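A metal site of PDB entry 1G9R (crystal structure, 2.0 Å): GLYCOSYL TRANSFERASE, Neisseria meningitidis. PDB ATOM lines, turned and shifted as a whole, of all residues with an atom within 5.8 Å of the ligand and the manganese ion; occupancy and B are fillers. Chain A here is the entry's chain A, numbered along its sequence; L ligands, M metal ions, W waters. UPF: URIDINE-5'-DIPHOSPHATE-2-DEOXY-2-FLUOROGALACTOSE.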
ATOM      1  N   PHE A   5       8.401   3.188 -24.716  1.00  0.00           N
ATOM      2  CA  PHE A   5       7.501   2.657 -23.694  1.00  0.00           C
ATOM      3  C   PHE A   5       6.369   2.027 -24.498  1.00  0.00           C
ATOM      4  O   PHE A   5       6.202   2.328 -25.690  1.00  0.00           O
ATOM      5  CB  PHE A   5       6.892   3.799 -22.851  1.00  0.00           C
ATOM      6  CG  PHE A   5       7.780   4.332 -21.767  1.00  0.00           C
ATOM      7  CD1 PHE A   5       8.109   3.540 -20.661  1.00  0.00           C
ATOM      8  CD2 PHE A   5       8.214   5.653 -21.794  1.00  0.00           C
ATOM      9  CE1 PHE A   5       8.858   4.075 -19.598  1.00  0.00           C
ATOM     10  CE2 PHE A   5       8.963   6.187 -20.731  1.00  0.00           C
ATOM     11  CZ  PHE A   5       9.276   5.394 -19.630  1.00  0.00           C
ATOM     12  N   ALA A   6       5.608   1.128 -23.869  1.00  0.00           N
ATOM     13  CA  ALA A   6       4.468   0.488 -24.520  1.00  0.00           C
ATOM     14  C   ALA A   6       3.368   0.527 -23.476  1.00  0.00           C
ATOM     15  O   ALA A   6       3.587   0.155 -22.312  1.00  0.00           O
ATOM     16  CB  ALA A   6       4.770  -0.971 -24.878  1.00  0.00           C
ATOM     17  N   ALA A   7       2.181   0.962 -23.873  1.00  0.00           N
ATOM     18  CA  ALA A   7       1.096   1.019 -22.900  1.00  0.00           C
ATOM     19  C   ALA A   7      -0.276   1.031 -23.541  1.00  0.00           C
ATOM     20  O   ALA A   7      -0.432   1.511 -24.658  1.00  0.00           O
ATOM     21  CB  ALA A   7       1.254   2.250 -22.002  1.00  0.00           C
ATOM     22  N   ASP A   8      -1.244   0.465 -22.823  1.00  0.00           N
ATOM     23  CA  ASP A   8      -2.633   0.479 -23.254  1.00  0.00           C
ATOM     24  C   ASP A   8      -3.272   1.573 -22.387  1.00  0.00           C
ATOM     25  O   ASP A   8      -2.600   2.157 -21.543  1.00  0.00           O
ATOM     26  CB  ASP A   8      -3.338  -0.870 -23.025  1.00  0.00           C
ATOM     27  CG  ASP A   8      -2.970  -1.509 -21.704  1.00  0.00           C
ATOM     28  OD1 ASP A   8      -2.659  -0.786 -20.727  1.00  0.00           O
ATOM     29  OD2 ASP A   8      -3.007  -2.758 -21.651  1.00  0.00           O
ATOM     30  N   ASN A  10      -5.155   1.483 -19.846  1.00  0.00           N
ATOM     31  CA  ASN A  10      -5.066   1.181 -18.421  1.00  0.00           C
ATOM     32  C   ASN A  10      -3.784   1.699 -17.767  1.00  0.00           C
ATOM     33  O   ASN A  10      -3.800   2.072 -16.585  1.00  0.00           O
ATOM     34  CB  ASN A  10      -5.161  -0.329 -18.206  1.00  0.00           C
ATOM     35  CG  ASN A  10      -5.104  -0.722 -16.743  1.00  0.00           C
ATOM     36  OD1 ASN A  10      -5.816  -0.152 -15.913  1.00  0.00           O
ATOM     37  ND2 ASN A  10      -4.263  -1.692 -16.417  1.00  0.00           N
ATOM     38  N   TYR A  11      -2.690   1.719 -18.510  1.00  0.00           N
ATOM     39  CA  TYR A  11      -1.408   2.167 -17.960  1.00  0.00           C
ATOM     40  C   TYR A  11      -0.994   3.583 -18.337  1.00  0.00           C
ATOM     41  O   TYR A  11       0.138   3.985 -18.071  1.00  0.00           O
ATOM     42  CB  TYR A  11      -0.294   1.205 -18.383  1.00  0.00           C
ATOM     43  CG  TYR A  11       0.024   0.128 -17.379  1.00  0.00           C
ATOM     44  CD1 TYR A  11      -0.941  -0.332 -16.474  1.00  0.00           C
ATOM     45  CD2 TYR A  11       1.294  -0.446 -17.330  1.00  0.00           C
ATOM     46  CE1 TYR A  11      -0.644  -1.333 -15.551  1.00  0.00           C
ATOM     47  CE2 TYR A  11       1.595  -1.453 -16.419  1.00  0.00           C
ATOM     48  CZ  TYR A  11       0.619  -1.887 -15.533  1.00  0.00           C
ATOM     49  OH  TYR A  11       0.937  -2.869 -14.629  1.00  0.00           O
ATOM     50  N   ILE A  76       0.266 -14.562 -17.001  1.00  0.00           N
ATOM     51  CA  ILE A  76       0.552 -13.674 -15.871  1.00  0.00           C
ATOM     52  C   ILE A  76      -0.552 -12.627 -15.799  1.00  0.00           C
ATOM     53  O   ILE A  76      -0.637 -11.719 -16.628  1.00  0.00           O
ATOM     54  CB  ILE A  76       1.931 -12.993 -16.022  1.00  0.00           C
ATOM     55  CG1 ILE A  76       3.014 -14.070 -16.235  1.00  0.00           C
ATOM     56  CG2 ILE A  76       2.268 -12.178 -14.768  1.00  0.00           C
ATOM     57  CD1 ILE A  76       4.441 -13.526 -16.356  1.00  0.00           C
ATOM     58  N   HIS A  78      -1.364  -9.849 -14.043  1.00  0.00           N
ATOM     59  CA  HIS A  78      -1.191  -8.394 -14.060  1.00  0.00           C
ATOM     60  C   HIS A  78      -0.642  -7.845 -15.366  1.00  0.00           C
ATOM     61  O   HIS A  78      -0.466  -6.645 -15.514  1.00  0.00           O
ATOM     62  CB  HIS A  78      -0.288  -7.925 -12.904  1.00  0.00           C
ATOM     63  CG  HIS A  78       1.155  -8.271 -13.071  1.00  0.00           C
ATOM     64  ND1 HIS A  78       1.692  -9.478 -12.693  1.00  0.00           N
ATOM     65  CD2 HIS A  78       2.192  -7.556 -13.595  1.00  0.00           C
ATOM     66  CE1 HIS A  78       2.981  -9.502 -12.974  1.00  0.00           C
ATOM     67  NE2 HIS A  78       3.313  -8.345 -13.523  1.00  0.00           N
ATOM     68  N   ILE A  79      -0.398  -8.723 -16.336  1.00  0.00           N
ATOM     69  CA  ILE A  79       0.129  -8.277 -17.619  1.00  0.00           C
ATOM     70  C   ILE A  79      -0.850  -8.379 -18.771  1.00  0.00           C
ATOM     71  O   ILE A  79      -1.413  -9.435 -19.027  1.00  0.00           O
ATOM     72  CB  ILE A  79       1.393  -9.075 -17.987  1.00  0.00           C
ATOM     73  CG1 ILE A  79       2.434  -8.942 -16.882  1.00  0.00           C
ATOM     74  CG2 ILE A  79       1.969  -8.571 -19.302  1.00  0.00           C
ATOM     75  CD1 ILE A  79       3.604  -9.907 -17.025  1.00  0.00           C
ATOM     76  N   SER A  80      -1.057  -7.262 -19.476  1.00  0.00           N
ATOM     77  CA  SER A  80      -1.960  -7.239 -20.620  1.00  0.00           C
ATOM     78  C   SER A  80      -1.187  -7.622 -21.888  1.00  0.00           C
ATOM     79  O   SER A  80       0.049  -7.708 -21.878  1.00  0.00           O
ATOM     80  CB  SER A  80      -2.562  -5.859 -20.786  1.00  0.00           C
ATOM     81  OG  SER A  80      -1.572  -4.938 -21.194  1.00  0.00           O
ATOM     82  N   THR A  82      -0.480  -6.009 -24.402  1.00  0.00           N
ATOM     83  CA  THR A  82       0.399  -4.946 -24.880  1.00  0.00           C
ATOM     84  C   THR A  82       1.892  -5.270 -24.659  1.00  0.00           C
ATOM     85  O   THR A  82       2.766  -4.747 -25.359  1.00  0.00           O
ATOM     86  CB  THR A  82       0.057  -3.606 -24.180  1.00  0.00           C
ATOM     87  OG1 THR A  82      -1.271  -3.213 -24.542  1.00  0.00           O
ATOM     88  CG2 THR A  82       1.029  -2.509 -24.587  1.00  0.00           C
ATOM     89  N   THR A  83       2.162  -6.124 -23.688  1.00  0.00           N
ATOM     90  CA  THR A  83       3.516  -6.542 -23.346  1.00  0.00           C
ATOM     91  C   THR A  83       4.285  -7.141 -24.551  1.00  0.00           C
ATOM     92  O   THR A  83       5.521  -7.162 -24.575  1.00  0.00           O
ATOM     93  CB  THR A  83       3.478  -7.573 -22.175  1.00  0.00           C
ATOM     94  OG1 THR A  83       4.795  -7.734 -21.614  1.00  0.00           O
ATOM     95  CG2 THR A  83       2.968  -8.918 -22.643  1.00  0.00           C
ATOM     96  N   ARG A  86       6.483  -4.896 -28.104  1.00  0.00           N
ATOM     97  CA  ARG A  86       7.913  -4.651 -28.256  1.00  0.00           C
ATOM     98  C   ARG A  86       8.540  -5.530 -29.342  1.00  0.00           C
ATOM     99  O   ARG A  86       9.563  -5.173 -29.922  1.00  0.00           O
ATOM    100  CB  ARG A  86       8.615  -4.850 -26.910  1.00  0.00           C
ATOM    101  CG  ARG A  86       8.592  -6.262 -26.373  1.00  0.00           C
ATOM    102  CD  ARG A  86       9.107  -6.288 -24.930  1.00  0.00           C
ATOM    103  NE  ARG A  86       8.023  -6.145 -23.960  1.00  0.00           N
ATOM    104  CZ  ARG A  86       8.199  -6.062 -22.637  1.00  0.00           C
ATOM    105  NH1 ARG A  86       9.428  -6.092 -22.133  1.00  0.00           N
ATOM    106  NH2 ARG A  86       7.144  -6.013 -21.826  1.00  0.00           N
ATOM    107  N   TYR A 101      14.419   0.711 -24.553  1.00  0.00           N
ATOM    108  CA  TYR A 101      13.083   0.312 -24.162  1.00  0.00           C
ATOM    109  C   TYR A 101      12.979   0.130 -22.656  1.00  0.00           C
ATOM    110  O   TYR A 101      13.842  -0.512 -22.030  1.00  0.00           O
ATOM    111  CB  TYR A 101      12.695  -1.012 -24.860  1.00  0.00           C
ATOM    112  CG  TYR A 101      11.440  -1.603 -24.257  1.00  0.00           C
ATOM    113  CD1 TYR A 101      10.173  -1.278 -24.747  1.00  0.00           C
ATOM    114  CD2 TYR A 101      11.509  -2.404 -23.115  1.00  0.00           C
ATOM    115  CE1 TYR A 101       9.009  -1.721 -24.110  1.00  0.00           C
ATOM    116  CE2 TYR A 101      10.358  -2.838 -22.461  1.00  0.00           C
ATOM    117  CZ  TYR A 101       9.120  -2.487 -22.964  1.00  0.00           C
ATOM    118  OH  TYR A 101       7.990  -2.897 -22.266  1.00  0.00           O
ATOM    119  N   LEU A 102      11.914   0.668 -22.075  1.00  0.00           N
ATOM    120  CA  LEU A 102      11.655   0.558 -20.641  1.00  0.00           C
ATOM    121  C   LEU A 102      10.224   0.091 -20.404  1.00  0.00           C
ATOM    122  O   LEU A 102       9.317   0.478 -21.143  1.00  0.00           O
ATOM    123  CB  LEU A 102      11.842   1.918 -19.953  1.00  0.00           C
ATOM    124  CG  LEU A 102      13.222   2.547 -20.027  1.00  0.00           C
ATOM    125  CD1 LEU A 102      13.185   3.911 -19.381  1.00  0.00           C
ATOM    126  CD2 LEU A 102      14.247   1.634 -19.345  1.00  0.00           C
ATOM    127  N   ASP A 103      10.027  -0.740 -19.383  1.00  0.00           N
ATOM    128  CA  ASP A 103       8.705  -1.208 -18.984  1.00  0.00           C
ATOM    129  C   ASP A 103       8.060   0.025 -18.335  1.00  0.00           C
ATOM    130  O   ASP A 103       8.747   0.998 -18.027  1.00  0.00           O
ATOM    131  CB  ASP A 103       8.812  -2.316 -17.941  1.00  0.00           C
ATOM    132  CG  ASP A 103       8.695  -3.718 -18.526  1.00  0.00           C
ATOM    133  OD1 ASP A 103       8.634  -4.675 -17.735  1.00  0.00           O
ATOM    134  OD2 ASP A 103       8.672  -3.880 -19.765  1.00  0.00           O
ATOM    135  N   ILE A 104       6.765  -0.031 -18.081  1.00  0.00           N
ATOM    136  CA  ILE A 104       6.063   1.102 -17.480  1.00  0.00           C
ATOM    137  C   ILE A 104       6.295   1.177 -15.975  1.00  0.00           C
ATOM    138  O   ILE A 104       6.286   2.266 -15.383  1.00  0.00           O
ATOM    139  CB  ILE A 104       4.552   0.988 -17.741  1.00  0.00           C
ATOM    140  CG1 ILE A 104       4.290   1.073 -19.242  1.00  0.00           C
ATOM    141  CG2 ILE A 104       3.787   2.058 -16.953  1.00  0.00           C
ATOM    142  CD1 ILE A 104       4.725   2.375 -19.901  1.00  0.00           C
ATOM    143  N   ASP A 105       6.505   0.018 -15.355  1.00  0.00           N
ATOM    144  CA  ASP A 105       6.721  -0.066 -13.913  1.00  0.00           C
ATOM    145  C   ASP A 105       8.175   0.167 -13.517  1.00  0.00           C
ATOM    146  O   ASP A 105       8.739  -0.614 -12.748  1.00  0.00           O
ATOM    147  CB  ASP A 105       6.261  -1.434 -13.402  1.00  0.00           C
ATOM    148  CG  ASP A 105       7.012  -2.587 -14.042  1.00  0.00           C
ATOM    149  OD1 ASP A 105       7.568  -2.396 -15.153  1.00  0.00           O
ATOM    150  OD2 ASP A 105       7.043  -3.685 -13.463  1.00  0.00           O
ATOM    151  N   VAL A 106       8.777   1.233 -14.038  1.00  0.00           N
ATOM    152  CA  VAL A 106      10.141   1.568 -13.676  1.00  0.00           C
ATOM    153  C   VAL A 106      10.194   2.989 -13.131  1.00  0.00           C
ATOM    154  O   VAL A 106       9.324   3.818 -13.408  1.00  0.00           O
ATOM    155  CB  VAL A 106      11.121   1.485 -14.886  1.00  0.00           C
ATOM    156  CG1 VAL A 106      11.027   0.117 -15.556  1.00  0.00           C
ATOM    157  CG2 VAL A 106      10.844   2.618 -15.865  1.00  0.00           C
ATOM    158  N   ASP A 130      18.269 -11.490 -15.188  1.00  0.00           N
ATOM    159  CA  ASP A 130      17.162 -11.707 -14.260  1.00  0.00           C
ATOM    160  C   ASP A 130      17.618 -12.771 -13.267  1.00  0.00           C
ATOM    161  O   ASP A 130      17.627 -13.965 -13.587  1.00  0.00           O
ATOM    162  CB  ASP A 130      15.909 -12.184 -15.002  1.00  0.00           C
ATOM    163  CG  ASP A 130      14.682 -12.146 -14.124  1.00  0.00           C
ATOM    164  OD1 ASP A 130      14.730 -12.685 -12.994  1.00  0.00           O
ATOM    165  OD2 ASP A 130      13.669 -11.571 -14.572  1.00  0.00           O
ATOM    166  N   ASN A 153      16.269  -9.968 -18.168  1.00  0.00           N
ATOM    167  CA  ASN A 153      14.937  -9.442 -17.901  1.00  0.00           C
ATOM    168  C   ASN A 153      14.610  -8.493 -19.057  1.00  0.00           C
ATOM    169  O   ASN A 153      15.448  -7.708 -19.476  1.00  0.00           O
ATOM    170  CB  ASN A 153      14.911  -8.710 -16.548  1.00  0.00           C
ATOM    171  CG  ASN A 153      13.536  -8.170 -16.212  1.00  0.00           C
ATOM    172  OD1 ASN A 153      13.220  -7.032 -16.522  1.00  0.00           O
ATOM    173  ND2 ASN A 153      12.711  -9.006 -15.603  1.00  0.00           N
ATOM    174  N   ALA A 154      13.383  -8.591 -19.567  1.00  0.00           N
ATOM    175  CA  ALA A 154      12.970  -7.761 -20.696  1.00  0.00           C
ATOM    176  C   ALA A 154      12.470  -6.359 -20.356  1.00  0.00           C
ATOM    177  O   ALA A 154      12.055  -5.605 -21.245  1.00  0.00           O
ATOM    178  CB  ALA A 154      11.899  -8.504 -21.487  1.00  0.00           C
ATOM    179  N   GLY A 155      12.509  -5.995 -19.078  1.00  0.00           N
ATOM    180  CA  GLY A 155      12.028  -4.685 -18.666  1.00  0.00           C
ATOM    181  C   GLY A 155      12.884  -3.477 -19.012  1.00  0.00           C
ATOM    182  O   GLY A 155      12.401  -2.340 -18.968  1.00  0.00           O
ATOM    183  N   TYR A 186       7.304 -17.078 -19.127  1.00  0.00           N
ATOM    184  CA  TYR A 186       7.433 -15.631 -19.064  1.00  0.00           C
ATOM    185  C   TYR A 186       7.093 -14.839 -20.315  1.00  0.00           C
ATOM    186  O   TYR A 186       7.655 -13.775 -20.564  1.00  0.00           O
ATOM    187  CB  TYR A 186       8.822 -15.275 -18.530  1.00  0.00           C
ATOM    188  CG  TYR A 186       9.092 -15.885 -17.172  1.00  0.00           C
ATOM    189  CD1 TYR A 186       9.879 -17.031 -17.054  1.00  0.00           C
ATOM    190  CD2 TYR A 186       8.529 -15.342 -16.012  1.00  0.00           C
ATOM    191  CE1 TYR A 186      10.096 -17.627 -15.805  1.00  0.00           C
ATOM    192  CE2 TYR A 186       8.739 -15.931 -14.761  1.00  0.00           C
ATOM    193  CZ  TYR A 186       9.527 -17.076 -14.676  1.00  0.00           C
ATOM    194  OH  TYR A 186       9.743 -17.664 -13.448  1.00  0.00           O
ATOM    195  N   GLN A 187       6.178 -15.366 -21.111  1.00  0.00           N
ATOM    196  CA  GLN A 187       5.667 -14.686 -22.293  1.00  0.00           C
ATOM    197  C   GLN A 187       6.710 -14.021 -23.214  1.00  0.00           C
ATOM    198  O   GLN A 187       7.634 -14.680 -23.693  1.00  0.00           O
ATOM    199  CB  GLN A 187       4.613 -13.681 -21.798  1.00  0.00           C
ATOM    200  CG  GLN A 187       3.632 -14.360 -20.825  1.00  0.00           C
ATOM    201  CD  GLN A 187       2.657 -13.418 -20.112  1.00  0.00           C
ATOM    202  OE1 GLN A 187       1.663 -13.863 -19.551  1.00  0.00           O
ATOM    203  NE2 GLN A 187       2.954 -12.118 -20.107  1.00  0.00           N
ATOM    204  N   ASP A 188       6.568 -12.723 -23.469  1.00  0.00           N
ATOM    205  CA  ASP A 188       7.485 -12.026 -24.365  1.00  0.00           C
ATOM    206  C   ASP A 188       8.954 -12.099 -23.951  1.00  0.00           C
ATOM    207  O   ASP A 188       9.867 -12.083 -24.786  1.00  0.00           O
ATOM    208  CB  ASP A 188       7.090 -10.559 -24.518  1.00  0.00           C
ATOM    209  CG  ASP A 188       7.090  -9.829 -23.196  1.00  0.00           C
ATOM    210  OD1 ASP A 188       6.143 -10.035 -22.405  1.00  0.00           O
ATOM    211  OD2 ASP A 188       8.042  -9.067 -22.939  1.00  0.00           O
ATOM    212  N   GLN A 189       9.177 -12.166 -22.641  1.00  0.00           N
ATOM    213  CA  GLN A 189      10.529 -12.243 -22.096  1.00  0.00           C
ATOM    214  C   GLN A 189      11.211 -13.531 -22.554  1.00  0.00           C
ATOM    215  O   GLN A 189      12.398 -13.533 -22.871  1.00  0.00           O
ATOM    216  CB  GLN A 189      10.449 -12.171 -20.567  1.00  0.00           C
ATOM    217  CG  GLN A 189      11.785 -12.111 -19.851  1.00  0.00           C
ATOM    218  CD  GLN A 189      11.594 -11.768 -18.386  1.00  0.00           C
ATOM    219  OE1 GLN A 189      11.720 -10.606 -17.988  1.00  0.00           O
ATOM    220  NE2 GLN A 189      11.248 -12.774 -17.580  1.00  0.00           N
ATOM    221  N   MET A 210      15.596  -5.062  -9.473  1.00  0.00           N
ATOM    222  CA  MET A 210      14.290  -5.600  -9.099  1.00  0.00           C
ATOM    223  C   MET A 210      14.254  -6.156  -7.679  1.00  0.00           C
ATOM    224  O   MET A 210      15.273  -6.212  -6.997  1.00  0.00           O
ATOM    225  CB  MET A 210      13.914  -6.703 -10.111  1.00  0.00           C
ATOM    226  CG  MET A 210      13.784  -6.185 -11.540  1.00  0.00           C
ATOM    227  SD  MET A 210      13.825  -7.587 -12.915  1.00  0.00           S
ATOM    228  CE  MET A 210      15.736  -7.766 -13.075  1.00  0.00           C
ATOM    229  N   HIS A 244      13.017  -1.297 -10.894  1.00  0.00           N
ATOM    230  CA  HIS A 244      12.036  -1.998 -11.710  1.00  0.00           C
ATOM    231  C   HIS A 244      11.177  -2.879 -10.797  1.00  0.00           C
ATOM    232  O   HIS A 244      11.657  -3.869 -10.245  1.00  0.00           O
ATOM    233  CB  HIS A 244      12.732  -2.852 -12.770  1.00  0.00           C
ATOM    234  CG  HIS A 244      11.796  -3.595 -13.666  1.00  0.00           C
ATOM    235  ND1 HIS A 244      12.229  -4.577 -14.544  1.00  0.00           N
ATOM    236  CD2 HIS A 244      10.454  -3.508 -13.829  1.00  0.00           C
ATOM    237  CE1 HIS A 244      11.182  -5.068 -15.194  1.00  0.00           C
ATOM    238  NE2 HIS A 244      10.098  -4.431 -14.780  1.00  0.00           N
ATOM    239  N   TYR A 245       9.906  -2.528 -10.676  1.00  0.00           N
ATOM    240  CA  TYR A 245       8.979  -3.254  -9.818  1.00  0.00           C
ATOM    241  C   TYR A 245       8.333  -4.445 -10.497  1.00  0.00           C
ATOM    242  O   TYR A 245       7.101  -4.579 -10.522  1.00  0.00           O
ATOM    243  CB  TYR A 245       7.934  -2.263  -9.305  1.00  0.00           C
ATOM    244  CG  TYR A 245       8.600  -1.150  -8.545  1.00  0.00           C
ATOM    245  CD1 TYR A 245       9.052  -1.348  -7.231  1.00  0.00           C
ATOM    246  CD2 TYR A 245       8.891   0.067  -9.156  1.00  0.00           C
ATOM    247  CE1 TYR A 245       9.779  -0.367  -6.564  1.00  0.00           C
ATOM    248  CE2 TYR A 245       9.623   1.055  -8.491  1.00  0.00           C
ATOM    249  CZ  TYR A 245      10.072   0.828  -7.196  1.00  0.00           C
ATOM    250  OH  TYR A 245      10.836   1.779  -6.542  1.00  0.00           O
ATOM    251  N   CYS A 246       9.196  -5.305 -11.031  1.00  0.00           N
ATOM    252  CA  CYS A 246       8.788  -6.518 -11.737  1.00  0.00           C
ATOM    253  C   CYS A 246       7.932  -7.342 -10.795  1.00  0.00           C
ATOM    254  O   CYS A 246       8.237  -7.466  -9.610  1.00  0.00           O
ATOM    255  CB  CYS A 246      10.053  -7.301 -12.139  1.00  0.00           C
ATOM    256  SG  CYS A 246       9.756  -8.691 -13.256  1.00  0.00           S
ATOM    257  N   GLY A 247       6.851  -7.919 -11.310  1.00  0.00           N
ATOM    258  CA  GLY A 247       5.991  -8.720 -10.464  1.00  0.00           C
ATOM    259  C   GLY A 247       4.684  -8.022 -10.107  1.00  0.00           C
ATOM    260  O   GLY A 247       4.498  -6.850 -10.426  1.00  0.00           O
ATOM    261  N   PRO A 248       3.768  -8.722  -9.426  1.00  0.00           N
ATOM    262  CA  PRO A 248       2.477  -8.171  -9.026  1.00  0.00           C
ATOM    263  C   PRO A 248       2.497  -6.925  -8.140  1.00  0.00           C
ATOM    264  O   PRO A 248       1.594  -6.097  -8.212  1.00  0.00           O
ATOM    265  CB  PRO A 248       1.807  -9.365  -8.334  1.00  0.00           C
ATOM    266  CG  PRO A 248       2.985 -10.055  -7.688  1.00  0.00           C
ATOM    267  CD  PRO A 248       3.991 -10.042  -8.815  1.00  0.00           C
ATOM    268  N   LYS A 250       3.132  -3.486  -7.429  1.00  0.00           N
ATOM    269  CA  LYS A 250       3.457  -2.242  -8.119  1.00  0.00           C
ATOM    270  C   LYS A 250       3.491  -1.030  -7.194  1.00  0.00           C
ATOM    271  O   LYS A 250       2.740  -0.953  -6.221  1.00  0.00           O
ATOM    272  CB  LYS A 250       2.438  -1.993  -9.237  1.00  0.00           C
ATOM    273  CG  LYS A 250       2.370  -3.108 -10.292  1.00  0.00           C
ATOM    274  CD  LYS A 250       3.713  -3.397 -10.948  1.00  0.00           C
ATOM    275  CE  LYS A 250       3.565  -4.459 -12.049  1.00  0.00           C
ATOM    276  NZ  LYS A 250       4.893  -5.018 -12.474  1.00  0.00           N
HETATM  277  N1  UPF L   1       1.132  -3.333 -19.758  1.00  0.00           N
HETATM  278  C2  UPF L   1       0.210  -2.353 -20.150  1.00  0.00           C
HETATM  279  N3  UPF L   1      -0.978  -2.393 -19.401  1.00  0.00           N
HETATM  280  C4  UPF L   1      -1.294  -3.299 -18.321  1.00  0.00           C
HETATM  281  C5  UPF L   1      -0.291  -4.266 -17.993  1.00  0.00           C
HETATM  282  C6  UPF L   1       0.845  -4.270 -18.677  1.00  0.00           C
HETATM  283  O2  UPF L   1       0.432  -1.556 -21.061  1.00  0.00           O
HETATM  284  O4  UPF L   1      -2.371  -3.213 -17.770  1.00  0.00           O
HETATM  285  C1D UPF L   1       2.530  -3.615 -20.349  1.00  0.00           C
HETATM  286  C2D UPF L   1       3.459  -2.509 -19.882  1.00  0.00           C
HETATM  287  O2' UPF L   1       4.156  -1.941 -20.999  1.00  0.00           O
HETATM  288  C3D UPF L   1       4.381  -3.206 -18.891  1.00  0.00           C
HETATM  289  C4D UPF L   1       4.597  -4.536 -19.596  1.00  0.00           C
HETATM  290  O4D UPF L   1       3.248  -4.814 -20.191  1.00  0.00           O
HETATM  291  O3D UPF L   1       5.618  -2.604 -18.555  1.00  0.00           O
HETATM  292  C5D UPF L   1       4.457  -5.922 -19.036  1.00  0.00           C
HETATM  293  O5D UPF L   1       4.401  -6.125 -17.570  1.00  0.00           O
HETATM  294  PA  UPF L   1       4.992  -5.525 -16.202  1.00  0.00           P
HETATM  295  O1A UPF L   1       5.868  -4.346 -16.351  1.00  0.00           O
HETATM  296  O2A UPF L   1       3.884  -5.307 -15.205  1.00  0.00           O
HETATM  297  O3A UPF L   1       5.708  -6.943 -16.228  1.00  0.00           O
HETATM  298  PB  UPF L   1       6.749  -7.700 -15.290  1.00  0.00           P
HETATM  299  O1B UPF L   1       7.778  -6.662 -15.063  1.00  0.00           O
HETATM  300  O2B UPF L   1       6.048  -8.056 -14.062  1.00  0.00           O
HETATM  301  O3B UPF L   1       7.374  -8.935 -16.028  1.00  0.00           O
HETATM  302  C1' UPF L   1       8.696  -9.584 -16.683  1.00  0.00           C
HETATM  303  C2' UPF L   1       9.291  -8.405 -17.549  1.00  0.00           C
HETATM  304  C3' UPF L   1       8.273  -7.594 -18.508  1.00  0.00           C
HETATM  305  C4' UPF L   1       7.507  -8.627 -19.394  1.00  0.00           C
HETATM  306  C5' UPF L   1       6.938  -9.733 -18.391  1.00  0.00           C
HETATM  307  C6' UPF L   1       6.372 -10.873 -19.221  1.00  0.00           C
HETATM  308  F2' UPF L   1       9.986  -7.474 -16.749  1.00  0.00           F
HETATM  309  O3' UPF L   1       9.004  -6.768 -19.359  1.00  0.00           O
HETATM  310  O4' UPF L   1       8.429  -9.208 -20.359  1.00  0.00           O
HETATM  311  O5' UPF L   1       7.986 -10.466 -17.564  1.00  0.00           O
HETATM  312  O6' UPF L   1       5.346 -10.757 -20.171  1.00  0.00           O
HETATM  313 MN    MN M   1       7.997  -4.556 -15.672  1.00  0.00          MN
HETATM  314  O   HOH W   1       6.746   0.057 -21.605  1.00  0.00           O
HETATM  315  O   HOH W   2       5.845 -11.099 -13.733  1.00  0.00           O
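O3D of the ligand is in hydrogen-bond range of N of Ile 104 (2.9 Å). An oxygen (O4) of the ligand is in hydrogen-bond range of the side-chain amide nitrogen of Asn 10 (2.8 Å). An oxygen (O2B) of the ligand sits at hydrogen-bond distance from a ring nitrogen (NE2) of His 78 (2.8 Å). O2 of the ligand lies within hydrogen-bond range of N of Asp 8, 3.2 Å away. OG1 of Thr 83 lies close to O6' of the ligand (3.4 Å). OD1 of Asp 8 sits at hydrogen-bond distance from N3 of the ligand (2.7 Å). The side-chain amide nitrogen (NE2) of Gln 187 is in hydrogen-bond range of an oxygen (O6') of the ligand, 2.8 Å away. The side-chain amino group (NZ) of Lys 250 lies within salt-bridge range of an oxygen (O2A) of the ligand (2.9 Å). SG of Cys 246 sits at hydrogen-bond distance from O3B of the ligand (3.7 Å). OD1 of Asp 188 is in hydrogen-bond range of O6' of the ligand, 2.5 Å away. An oxygen (O3') of the ligand sits at hydrogen-bond distance from the guanidinium group (NH1) of Arg 86 (2.9 Å). The side-chain hydroxyl (OG) of Ser 80 sits at hydrogen-bond distance from a nitrogen (N3) of the ligand (3.2 Å). The backbone NH of Gly 247 is in hydrogen-bond range of an oxygen (O2B) of the ligand, at 2.9 Å. The backbone carbonyl oxygen (O) of Ala 6 sits at hydrogen-bond distance from an oxygen (O2') of the ligand, at 2.5 Å.
The guanidinium group of Arg 86 sits close to the side-chain hydroxyl of Tyr 101 (3.3 Å). OD1 of Asn 153 is in hydrogen-bond range of N of Gly 155. ND1 of His 244 sits close to OD1 of Asn 153, at 3.3 Å. The guanidinium group (NH1) of Arg 86 lies within hydrogen-bond range of the backbone carbonyl oxygen (O) of Ala 154 (2.8 Å). The backbone carbonyl oxygen of Gly 155 sits at hydrogen-bond distance from the backbone NH of Asp 103 (2.9 Å). O of Asp 105 sits at hydrogen-bond distance from N of Tyr 245 (3.1 Å). NZ of Lys 250 is in hydrogen-bond range of O of Tyr 245 (3.0 Å). The side-chain amide nitrogen (ND2) of Asn 153 sits at hydrogen-bond distance from the side-chain amide oxygen (OE1) of Gln 189 (3.0 Å).
A fluorine (F2') of the ligand lies close to the side-chain amide oxygen (OD1) of Asn 153 (3.3 Å). Merely in contact with the ligand: Ala 7, Tyr 11, Ile 79, Thr 82, Ala 154, Gly 155, Tyr 186 and Gln 189. Hydrophobic or aromatic side chains within 4 Å of the ligand: Tyr 11, His 78, Ile 79, Ile 104, Ala 154 and His 244. Of the 34 residues printed, 25 come within 4 Å of the ligand. The nearest printed residue that does not touch the ligand is Tyr 101 (4.1 Å).
Three residues have an atom within 4 Å of the manganese ion: Asp 103, Asp 105 and His 244.
The manganese ion is bound by the side-chain carboxylate (OD1) of Asp 103 (2.2 Å), an oxygen (O1B) of the ligand (2.2 Å), an oxygen (O1A) of the ligand (2.2 Å), the side-chain carboxylate (OD1) of Asp 105 (2.3 Å), a ring nitrogen (NE2) of His 244 (2.3 Å) and the side-chain carboxylate (OD2) of Asp 105 (2.6 Å).
Water W1 lies within hydrogen-bond range of O of Leu 102 (2.6 Å), N of Ala 6 (2.8 Å), OH of Tyr 101 (3.3 Å) and O2' of the ligand (3.3 Å).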
